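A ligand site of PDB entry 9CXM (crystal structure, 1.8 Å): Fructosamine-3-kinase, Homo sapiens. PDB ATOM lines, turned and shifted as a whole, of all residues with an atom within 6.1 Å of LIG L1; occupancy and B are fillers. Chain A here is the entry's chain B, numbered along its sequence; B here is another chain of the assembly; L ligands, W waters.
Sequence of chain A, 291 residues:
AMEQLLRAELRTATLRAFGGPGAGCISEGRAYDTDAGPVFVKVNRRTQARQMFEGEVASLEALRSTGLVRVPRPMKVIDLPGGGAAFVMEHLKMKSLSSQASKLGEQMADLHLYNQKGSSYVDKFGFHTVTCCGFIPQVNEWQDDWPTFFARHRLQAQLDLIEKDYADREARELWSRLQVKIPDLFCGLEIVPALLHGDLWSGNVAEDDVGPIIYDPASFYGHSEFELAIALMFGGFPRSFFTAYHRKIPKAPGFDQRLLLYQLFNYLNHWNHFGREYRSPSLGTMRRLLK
The side-chain carboxylate (OD2) of Asp 199 is in hydrogen-bond range of an oxygen (O6) of LIG L1, at 2.5 Å.
ND2 of Asn 269 lies within hydrogen-bond range of O4 of LIG L1 (2.8 Å).
An oxygen (O3) of LIG L1 lies close to a ring nitrogen (NE2) of His 270.
O5 of LIG L1 is in hydrogen-bond range of N of Gly 134 (3.3 Å).
O6 of LIG L1 lies within hydrogen-bond range of NE1 of Trp 201 (3.3 Å).
An oxygen (O3) of LG2 L2 lies within hydrogen-bond range of the indole nitrogen of Trp 201, 3.1 Å away.
The backbone NH (N) of Ile 26 is in hydrogen-bond range of an oxygen (O5) of LG2 L2.
An oxygen (O3) of LG2 L2 lies close to the side-chain amide oxygen of Asn 204.
O2 of LG2 L2 lies close to OD2 of Asp 216 (2.9 Å).
The backbone NH (N) of Cys 25 is in hydrogen-bond range of an oxygen (O1) of LG2 L2.
The side-chain sulfur (SG) of Cys 25 lies close to an oxygen (O1) of LG2 L2, at 3.7 Å.
An oxygen (O6) of LIG L1 lies within hydrogen-bond range of an oxygen (O2) of LG2 L2, at 2.6 Å.
O of Asp 199 lies within hydrogen-bond range of ND2 of Asn 204, at 2.9 Å.
The backbone carbonyl oxygen (O) of Asn 269 is in hydrogen-bond range of a ring nitrogen (ND1) of His 273.
The side-chain amide nitrogen (ND2) of Asn 269 lies within hydrogen-bond range of the side-chain sulfur (SG) of Cys 133.
The indole nitrogen (NE1) of Trp 201 sits close to the side-chain amide nitrogen (ND2) of Asn 204.
O of Cys 133 sits close to NE2 of His 273, 3.4 Å away.
The backbone NH (N) of Phe 135 is in hydrogen-bond range of a ring nitrogen (NE2) of His 273.
The side-chain amide oxygen (OD1) of Asn 204 sits close to the side-chain carboxylate (OD2) of Asp 216, 3.3 Å away.
Merely in contact with LIG L1: Phe 274 (3.4 Å), His 273 (3.7 Å), Phe 234 (3.8 Å), Ile 26 (3.8 Å), Asn 204 (3.8 Å), Asp 216 (3.8 Å), Cys 133 (3.9 Å) and Cys 25 (3.96 Å).
Hydrophobic or aromatic side chains that line LIG L1: Ile 26, Trp 201, Phe 234, His 270, His 273 and Phe 274.
Water W2 lies within hydrogen-bond range of O5 of LIG L1, O2 of LG2 L2 and OD1 of Asp 216.
Water W1 lies within hydrogen-bond range of OD1 of Asp 199 (2.8 Å) and O4 of LIG L1 (2.8 Å).
Water W3 lies within hydrogen-bond range of an oxygen (O5) of LIG L1 (2.9 Å), the backbone NH (N) of Gly 134 (3.1 Å) and the backbone carbonyl oxygen (O) of Cys 132 (3.4 Å).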
ATOM      1  N   CYS A  25     -31.777  -9.717 -34.113  1.00  0.00           N
ATOM      2  CA  CYS A  25     -31.879  -8.410 -33.439  1.00  0.00           C
ATOM      3  C   CYS A  25     -30.617  -7.574 -33.539  1.00  0.00           C
ATOM      4  O   CYS A  25     -30.596  -6.437 -33.063  1.00  0.00           O
ATOM      5  CB  CYS A  25     -32.250  -8.542 -31.947  1.00  0.00           C
ATOM      6  SG  CYS A  25     -33.738  -9.408 -31.485  1.00  0.00           S
ATOM      7  N   ILE A  26     -29.565  -8.104 -34.140  1.00  0.00           N
ATOM      8  CA  ILE A  26     -28.277  -7.443 -34.203  1.00  0.00           C
ATOM      9  C   ILE A  26     -27.938  -7.067 -35.623  1.00  0.00           C
ATOM     10  O   ILE A  26     -27.557  -5.926 -35.908  1.00  0.00           O
ATOM     11  CB  ILE A  26     -27.175  -8.344 -33.579  1.00  0.00           C
ATOM     12  CG1 ILE A  26     -27.432  -8.603 -32.078  1.00  0.00           C
ATOM     13  CG2 ILE A  26     -25.791  -7.747 -33.779  1.00  0.00           C
ATOM     14  CD1 ILE A  26     -27.452  -7.256 -31.269  1.00  0.00           C
ATOM     15  N   CYS A 132     -17.772 -10.515 -29.299  1.00  0.00           N
ATOM     16  CA  CYS A 132     -18.662  -9.411 -28.950  1.00  0.00           C
ATOM     17  C   CYS A 132     -19.913  -9.981 -28.332  1.00  0.00           C
ATOM     18  O   CYS A 132     -20.405 -11.033 -28.737  1.00  0.00           O
ATOM     19  CB  CYS A 132     -19.021  -8.529 -30.162  1.00  0.00           C
ATOM     20  SG  CYS A 132     -17.713  -7.542 -30.639  1.00  0.00           S
ATOM     21  N   CYS A 133     -20.376  -9.345 -27.274  1.00  0.00           N
ATOM     22  CA  CYS A 133     -21.702  -9.637 -26.781  1.00  0.00           C
ATOM     23  C   CYS A 133     -22.624  -8.762 -27.620  1.00  0.00           C
ATOM     24  O   CYS A 133     -22.719  -7.567 -27.353  1.00  0.00           O
ATOM     25  CB  CYS A 133     -21.829  -9.246 -25.316  1.00  0.00           C
ATOM     26  SG  CYS A 133     -23.294  -9.983 -24.596  1.00  0.00           S
ATOM     27  N   GLY A 134     -23.296  -9.336 -28.629  1.00  0.00           N
ATOM     28  CA  GLY A 134     -24.095  -8.464 -29.498  1.00  0.00           C
ATOM     29  C   GLY A 134     -23.229  -7.402 -30.165  1.00  0.00           C
ATOM     30  O   GLY A 134     -22.276  -7.708 -30.893  1.00  0.00           O
ATOM     31  N   PHE A 135     -23.561  -6.130 -29.929  1.00  0.00           N
ATOM     32  CA  PHE A 135     -22.777  -5.020 -30.453  1.00  0.00           C
ATOM     33  C   PHE A 135     -21.583  -4.714 -29.571  1.00  0.00           C
ATOM     34  O   PHE A 135     -20.732  -3.917 -29.979  1.00  0.00           O
ATOM     35  CB  PHE A 135     -23.585  -3.685 -30.486  1.00  0.00           C
ATOM     36  CG  PHE A 135     -24.764  -3.693 -31.372  1.00  0.00           C
ATOM     37  CD1 PHE A 135     -24.618  -3.983 -32.734  1.00  0.00           C
ATOM     38  CD2 PHE A 135     -26.014  -3.370 -30.895  1.00  0.00           C
ATOM     39  CE1 PHE A 135     -25.733  -3.997 -33.607  1.00  0.00           C
ATOM     40  CE2 PHE A 135     -27.124  -3.361 -31.753  1.00  0.00           C
ATOM     41  CZ  PHE A 135     -26.981  -3.663 -33.109  1.00  0.00           C
ATOM     42  N   ASP A 199     -23.945 -17.730 -26.188  1.00  0.00           N
ATOM     43  CA  ASP A 199     -25.209 -16.996 -26.447  1.00  0.00           C
ATOM     44  C   ASP A 199     -26.314 -17.989 -26.794  1.00  0.00           C
ATOM     45  O   ASP A 199     -27.035 -17.847 -27.793  1.00  0.00           O
ATOM     46  CB  ASP A 199     -24.981 -15.963 -27.555  1.00  0.00           C
ATOM     47  CG  ASP A 199     -26.154 -14.948 -27.672  1.00  0.00           C
ATOM     48  OD1 ASP A 199     -26.883 -14.743 -26.695  1.00  0.00           O
ATOM     49  OD2 ASP A 199     -26.305 -14.385 -28.770  1.00  0.00           O
ATOM     50  N   TRP A 201     -29.374 -18.730 -26.404  1.00  0.00           N
ATOM     51  CA  TRP A 201     -30.804 -18.545 -26.220  1.00  0.00           C
ATOM     52  C   TRP A 201     -31.547 -19.352 -27.264  1.00  0.00           C
ATOM     53  O   TRP A 201     -30.972 -19.815 -28.248  1.00  0.00           O
ATOM     54  CB  TRP A 201     -31.182 -17.066 -26.252  1.00  0.00           C
ATOM     55  CG  TRP A 201     -31.241 -16.372 -27.523  1.00  0.00           C
ATOM     56  CD1 TRP A 201     -30.179 -15.993 -28.308  1.00  0.00           C
ATOM     57  CD2 TRP A 201     -32.452 -15.839 -28.186  1.00  0.00           C
ATOM     58  NE1 TRP A 201     -30.652 -15.280 -29.454  1.00  0.00           N
ATOM     59  CE2 TRP A 201     -32.027 -15.208 -29.394  1.00  0.00           C
ATOM     60  CE3 TRP A 201     -33.824 -15.851 -27.889  1.00  0.00           C
ATOM     61  CZ2 TRP A 201     -32.932 -14.562 -30.312  1.00  0.00           C
ATOM     62  CZ3 TRP A 201     -34.698 -15.204 -28.764  1.00  0.00           C
ATOM     63  CH2 TRP A 201     -34.247 -14.563 -29.958  1.00  0.00           C
ATOM     64  N   ASN A 204     -31.102 -19.107 -30.982  1.00  0.00           N
ATOM     65  CA  ASN A 204     -29.809 -19.441 -31.580  1.00  0.00           C
ATOM     66  C   ASN A 204     -29.621 -20.940 -31.660  1.00  0.00           C
ATOM     67  O   ASN A 204     -28.485 -21.415 -31.949  1.00  0.00           O
ATOM     68  CB  ASN A 204     -28.623 -18.799 -30.793  1.00  0.00           C
ATOM     69  CG  ASN A 204     -28.452 -17.332 -31.122  1.00  0.00           C
ATOM     70  OD1 ASN A 204     -29.010 -16.842 -32.140  1.00  0.00           O
ATOM     71  ND2 ASN A 204     -27.651 -16.590 -30.293  1.00  0.00           N
ATOM     72  N   ASP A 216     -24.618 -18.399 -34.261  1.00  0.00           N
ATOM     73  CA  ASP A 216     -24.459 -17.080 -33.640  1.00  0.00           C
ATOM     74  C   ASP A 216     -23.725 -17.165 -32.278  1.00  0.00           C
ATOM     75  O   ASP A 216     -24.173 -16.509 -31.310  1.00  0.00           O
ATOM     76  CB  ASP A 216     -25.841 -16.488 -33.414  1.00  0.00           C
ATOM     77  CG  ASP A 216     -25.822 -14.954 -33.159  1.00  0.00           C
ATOM     78  OD1 ASP A 216     -24.817 -14.290 -33.509  1.00  0.00           O
ATOM     79  OD2 ASP A 216     -26.841 -14.450 -32.651  1.00  0.00           O
ATOM     80  N   ILE A 230     -28.958 -17.984 -20.037  1.00  0.00           N
ATOM     81  CA  ILE A 230     -29.783 -17.344 -21.069  1.00  0.00           C
ATOM     82  C   ILE A 230     -30.810 -18.339 -21.642  1.00  0.00           C
ATOM     83  O   ILE A 230     -31.908 -17.932 -22.028  1.00  0.00           O
ATOM     84  CB  ILE A 230     -28.927 -16.702 -22.174  1.00  0.00           C
ATOM     85  CG1 ILE A 230     -29.782 -15.713 -23.017  1.00  0.00           C
ATOM     86  CG2 ILE A 230     -28.245 -17.818 -23.032  1.00  0.00           C
ATOM     87  CD1 ILE A 230     -29.023 -14.913 -23.933  1.00  0.00           C
ATOM     88  N   PHE A 234     -35.015 -16.907 -21.062  1.00  0.00           N
ATOM     89  CA  PHE A 234     -35.914 -16.554 -22.166  1.00  0.00           C
ATOM     90  C   PHE A 234     -36.754 -17.725 -22.656  1.00  0.00           C
ATOM     91  O   PHE A 234     -37.560 -17.524 -23.567  1.00  0.00           O
ATOM     92  CB  PHE A 234     -35.141 -15.934 -23.315  1.00  0.00           C
ATOM     93  CG  PHE A 234     -34.483 -14.596 -22.966  1.00  0.00           C
ATOM     94  CD1 PHE A 234     -35.208 -13.542 -22.358  1.00  0.00           C
ATOM     95  CD2 PHE A 234     -33.117 -14.441 -23.096  1.00  0.00           C
ATOM     96  CE1 PHE A 234     -34.573 -12.298 -22.027  1.00  0.00           C
ATOM     97  CE2 PHE A 234     -32.473 -13.237 -22.759  1.00  0.00           C
ATOM     98  CZ  PHE A 234     -33.210 -12.154 -22.206  1.00  0.00           C
ATOM     99  N   ASN A 269     -26.879  -6.831 -20.068  1.00  0.00           N
ATOM    100  CA  ASN A 269     -26.573  -6.729 -21.476  1.00  0.00           C
ATOM    101  C   ASN A 269     -27.798  -6.326 -22.278  1.00  0.00           C
ATOM    102  O   ASN A 269     -27.685  -5.573 -23.252  1.00  0.00           O
ATOM    103  CB  ASN A 269     -26.042  -8.094 -21.951  1.00  0.00           C
ATOM    104  CG  ASN A 269     -25.592  -8.062 -23.384  1.00  0.00           C
ATOM    105  OD1 ASN A 269     -24.716  -7.287 -23.778  1.00  0.00           O
ATOM    106  ND2 ASN A 269     -26.166  -8.949 -24.178  1.00  0.00           N
ATOM    107  N   HIS A 270     -28.975  -6.814 -21.885  1.00  0.00           N
ATOM    108  CA  HIS A 270     -30.191  -6.399 -22.601  1.00  0.00           C
ATOM    109  C   HIS A 270     -30.573  -4.968 -22.260  1.00  0.00           C
ATOM    110  O   HIS A 270     -31.156  -4.268 -23.087  1.00  0.00           O
ATOM    111  CB  HIS A 270     -31.341  -7.360 -22.253  1.00  0.00           C
ATOM    112  CG  HIS A 270     -31.308  -8.625 -23.073  1.00  0.00           C
ATOM    113  ND1 HIS A 270     -30.229  -9.504 -23.028  1.00  0.00           N
ATOM    114  CD2 HIS A 270     -32.129  -9.078 -24.041  1.00  0.00           C
ATOM    115  CE1 HIS A 270     -30.426 -10.471 -23.921  1.00  0.00           C
ATOM    116  NE2 HIS A 270     -31.575 -10.238 -24.552  1.00  0.00           N
ATOM    117  N   HIS A 273     -28.276  -3.137 -24.588  1.00  0.00           N
ATOM    118  CA  HIS A 273     -28.667  -3.235 -26.009  1.00  0.00           C
ATOM    119  C   HIS A 273     -30.020  -2.600 -26.306  1.00  0.00           C
ATOM    120  O   HIS A 273     -30.207  -1.988 -27.374  1.00  0.00           O
ATOM    121  CB  HIS A 273     -28.701  -4.694 -26.417  1.00  0.00           C
ATOM    122  CG  HIS A 273     -27.385  -5.197 -26.851  1.00  0.00           C
ATOM    123  ND1 HIS A 273     -26.475  -5.744 -25.959  1.00  0.00           N
ATOM    124  CD2 HIS A 273     -26.766  -5.190 -28.067  1.00  0.00           C
ATOM    125  CE1 HIS A 273     -25.382  -6.092 -26.619  1.00  0.00           C
ATOM    126  NE2 HIS A 273     -25.543  -5.786 -27.902  1.00  0.00           N
ATOM    127  N   PHE A 274     -31.005  -2.831 -25.447  1.00  0.00           N
ATOM    128  CA  PHE A 274     -32.402  -2.592 -25.779  1.00  0.00           C
ATOM    129  C   PHE A 274     -33.085  -1.586 -24.882  1.00  0.00           C
ATOM    130  O   PHE A 274     -34.274  -1.353 -25.095  1.00  0.00           O
ATOM    131  CB  PHE A 274     -33.197  -3.914 -25.764  1.00  0.00           C
ATOM    132  CG  PHE A 274     -32.608  -4.971 -26.626  1.00  0.00           C
ATOM    133  CD1 PHE A 274     -32.474  -4.747 -27.985  1.00  0.00           C
ATOM    134  CD2 PHE A 274     -32.126  -6.166 -26.097  1.00  0.00           C
ATOM    135  CE1 PHE A 274     -31.947  -5.689 -28.828  1.00  0.00           C
ATOM    136  CE2 PHE A 274     -31.598  -7.129 -26.962  1.00  0.00           C
ATOM    137  CZ  PHE A 274     -31.493  -6.874 -28.306  1.00  0.00           C
ATOM    138  N   TYR A 278     -35.170  -3.045 -19.439  1.00  0.00           N
ATOM    139  CA  TYR A 278     -34.460  -4.089 -18.709  1.00  0.00           C
ATOM    140  C   TYR A 278     -33.853  -3.586 -17.405  1.00  0.00           C
ATOM    141  O   TYR A 278     -33.148  -4.338 -16.729  1.00  0.00           O
ATOM    142  CB  TYR A 278     -33.421  -4.732 -19.626  1.00  0.00           C
ATOM    143  CG  TYR A 278     -34.056  -5.657 -20.675  1.00  0.00           C
ATOM    144  CD1 TYR A 278     -34.408  -6.960 -20.361  1.00  0.00           C
ATOM    145  CD2 TYR A 278     -34.269  -5.219 -21.996  1.00  0.00           C
ATOM    146  CE1 TYR A 278     -34.948  -7.817 -21.310  1.00  0.00           C
ATOM    147  CE2 TYR A 278     -34.857  -6.053 -22.937  1.00  0.00           C
ATOM    148  CZ  TYR A 278     -35.176  -7.344 -22.587  1.00  0.00           C
ATOM    149  OH  TYR A 278     -35.729  -8.152 -23.541  1.00  0.00           O
ATOM    150  N   SER B  27     -39.361  -7.551 -29.221  1.00  0.00           N
ATOM    151  CA  SER B  27     -39.273  -7.999 -27.836  1.00  0.00           C
ATOM    152  C   SER B  27     -39.842  -9.406 -27.678  1.00  0.00           C
ATOM    153  O   SER B  27     -41.040  -9.562 -27.423  1.00  0.00           O
ATOM    154  CB  SER B  27     -40.007  -7.037 -26.905  1.00  0.00           C
ATOM    155  OG  SER B  27     -39.554  -5.698 -27.057  1.00  0.00           O
ATOM    156  N   GLU B  28     -38.964 -10.425 -27.820  1.00  0.00           N
ATOM    157  CA  GLU B  28     -39.315 -11.843 -27.608  1.00  0.00           C
ATOM    158  C   GLU B  28     -40.568 -12.231 -28.393  1.00  0.00           C
ATOM    159  O   GLU B  28     -41.449 -12.936 -27.890  1.00  0.00           O
ATOM    160  CB  GLU B  28     -39.473 -12.158 -26.123  1.00  0.00           C
HETATM  161  N1  LIG L   1     -32.161 -11.787 -27.477  1.00  0.00           N
HETATM  162  C1  LIG L   1     -30.703 -12.118 -27.482  1.00  0.00           C
HETATM  163  C2  LIG L   1     -29.744 -11.393 -28.515  1.00  0.00           C
HETATM  164  O1  LIG L   1     -30.060 -10.468 -29.274  1.00  0.00           O
HETATM  165  C3  LIG L   1     -32.837 -12.568 -26.434  1.00  0.00           C
HETATM  166  C4  LIG L   1     -34.213 -12.012 -26.033  1.00  0.00           C
HETATM  167  C5  LIG L   1     -34.073 -10.145 -27.600  1.00  0.00           C
HETATM  168  C6  LIG L   1     -32.552 -10.386 -27.582  1.00  0.00           C
HETATM  169  C7  LIG L   1     -28.268 -11.859 -28.504  1.00  0.00           C
HETATM  170  C8  LIG L   1     -27.277 -10.733 -28.930  1.00  0.00           C
HETATM  171  C9  LIG L   1     -27.059  -9.578 -27.897  1.00  0.00           C
HETATM  172  C10 LIG L   1     -28.277  -8.734 -27.686  1.00  0.00           C
HETATM  173  O2  LIG L   1     -34.810 -11.275 -27.156  1.00  0.00           O
HETATM  174  O3  LIG L   1     -29.185  -9.545 -26.953  1.00  0.00           O
HETATM  175  O4  LIG L   1     -26.624 -10.160 -26.647  1.00  0.00           O
HETATM  176  O5  LIG L   1     -25.963 -11.269 -29.096  1.00  0.00           O
HETATM  177  O6  LIG L   1     -28.287 -12.925 -29.430  1.00  0.00           O
HETATM  178  P1  LG2 L   2     -29.609 -12.384 -32.391  1.00  0.00           P
HETATM  179  O1  LG2 L   2     -30.714 -11.482 -31.925  1.00  0.00           O
HETATM  180  O2  LG2 L   2     -28.161 -12.003 -31.884  1.00  0.00           O
HETATM  181  O3  LG2 L   2     -29.799 -13.859 -32.055  1.00  0.00           O
HETATM  182  P2  LG2 L   2     -28.440 -11.953 -35.141  1.00  0.00           P
HETATM  183  O4  LG2 L   2     -27.031 -11.926 -34.575  1.00  0.00           O
HETATM  184  O5  LG2 L   2     -28.796 -10.635 -35.844  1.00  0.00           O
HETATM  185  O6  LG2 L   2     -29.497 -12.310 -34.031  1.00  0.00           O
HETATM  186  P3  LG2 L   2     -28.594 -14.773 -36.067  1.00  0.00           P
HETATM  187  O7  LG2 L   2     -27.233 -15.294 -36.396  1.00  0.00           O
HETATM  188  O8  LG2 L   2     -29.269 -15.205 -34.794  1.00  0.00           O
HETATM  189  O9  LG2 L   2     -28.638 -13.176 -36.170  1.00  0.00           O
HETATM  190  O10 LG2 L   2     -29.540 -15.160 -37.280  1.00  0.00           O
HETATM  191  C1  LG2 L   2     -30.916 -14.695 -37.342  1.00  0.00           C
HETATM  192  C2  LG2 L   2     -31.771 -15.792 -37.928  1.00  0.00           C
HETATM  193  O11 LG2 L   2     -31.274 -16.156 -39.240  1.00  0.00           O
HETATM  194  C3  LG2 L   2     -31.792 -17.085 -37.135  1.00  0.00           C
HETATM  195  O12 LG2 L   2     -32.763 -17.112 -36.093  1.00  0.00           O
HETATM  196  C4  LG2 L   2     -32.127 -18.124 -38.213  1.00  0.00           C
HETATM  197  O13 LG2 L   2     -33.537 -18.132 -38.431  1.00  0.00           O
HETATM  198  C5  LG2 L   2     -31.423 -17.540 -39.453  1.00  0.00           C
HETATM  199  N1  LG2 L   2     -30.096 -18.089 -39.698  1.00  0.00           N
HETATM  200  C6  LG2 L   2     -28.950 -17.795 -39.007  1.00  0.00           C
HETATM  201  N2  LG2 L   2     -27.872 -18.407 -39.449  1.00  0.00           N
HETATM  202  C7  LG2 L   2     -28.352 -19.148 -40.522  1.00  0.00           C
HETATM  203  C8  LG2 L   2     -27.697 -19.992 -41.434  1.00  0.00           C
HETATM  204  N3  LG2 L   2     -26.392 -20.247 -41.393  1.00  0.00           N
HETATM  205  N4  LG2 L   2     -28.454 -20.581 -42.400  1.00  0.00           N
HETATM  206  C9  LG2 L   2     -29.770 -20.297 -42.455  1.00  0.00           C
HETATM  207  N5  LG2 L   2     -30.489 -19.520 -41.644  1.00  0.00           N
HETATM  208  C10 LG2 L   2     -29.715 -18.955 -40.699  1.00  0.00           C
HETATM  209  O   HOH W   1     -27.911 -12.414 -25.639  1.00  0.00           O
HETATM  210  O   HOH W   2     -25.038 -11.793 -31.557  1.00  0.00           O
HETATM  211  O   HOH W   3     -23.472 -12.391 -28.126  1.00  0.00           O
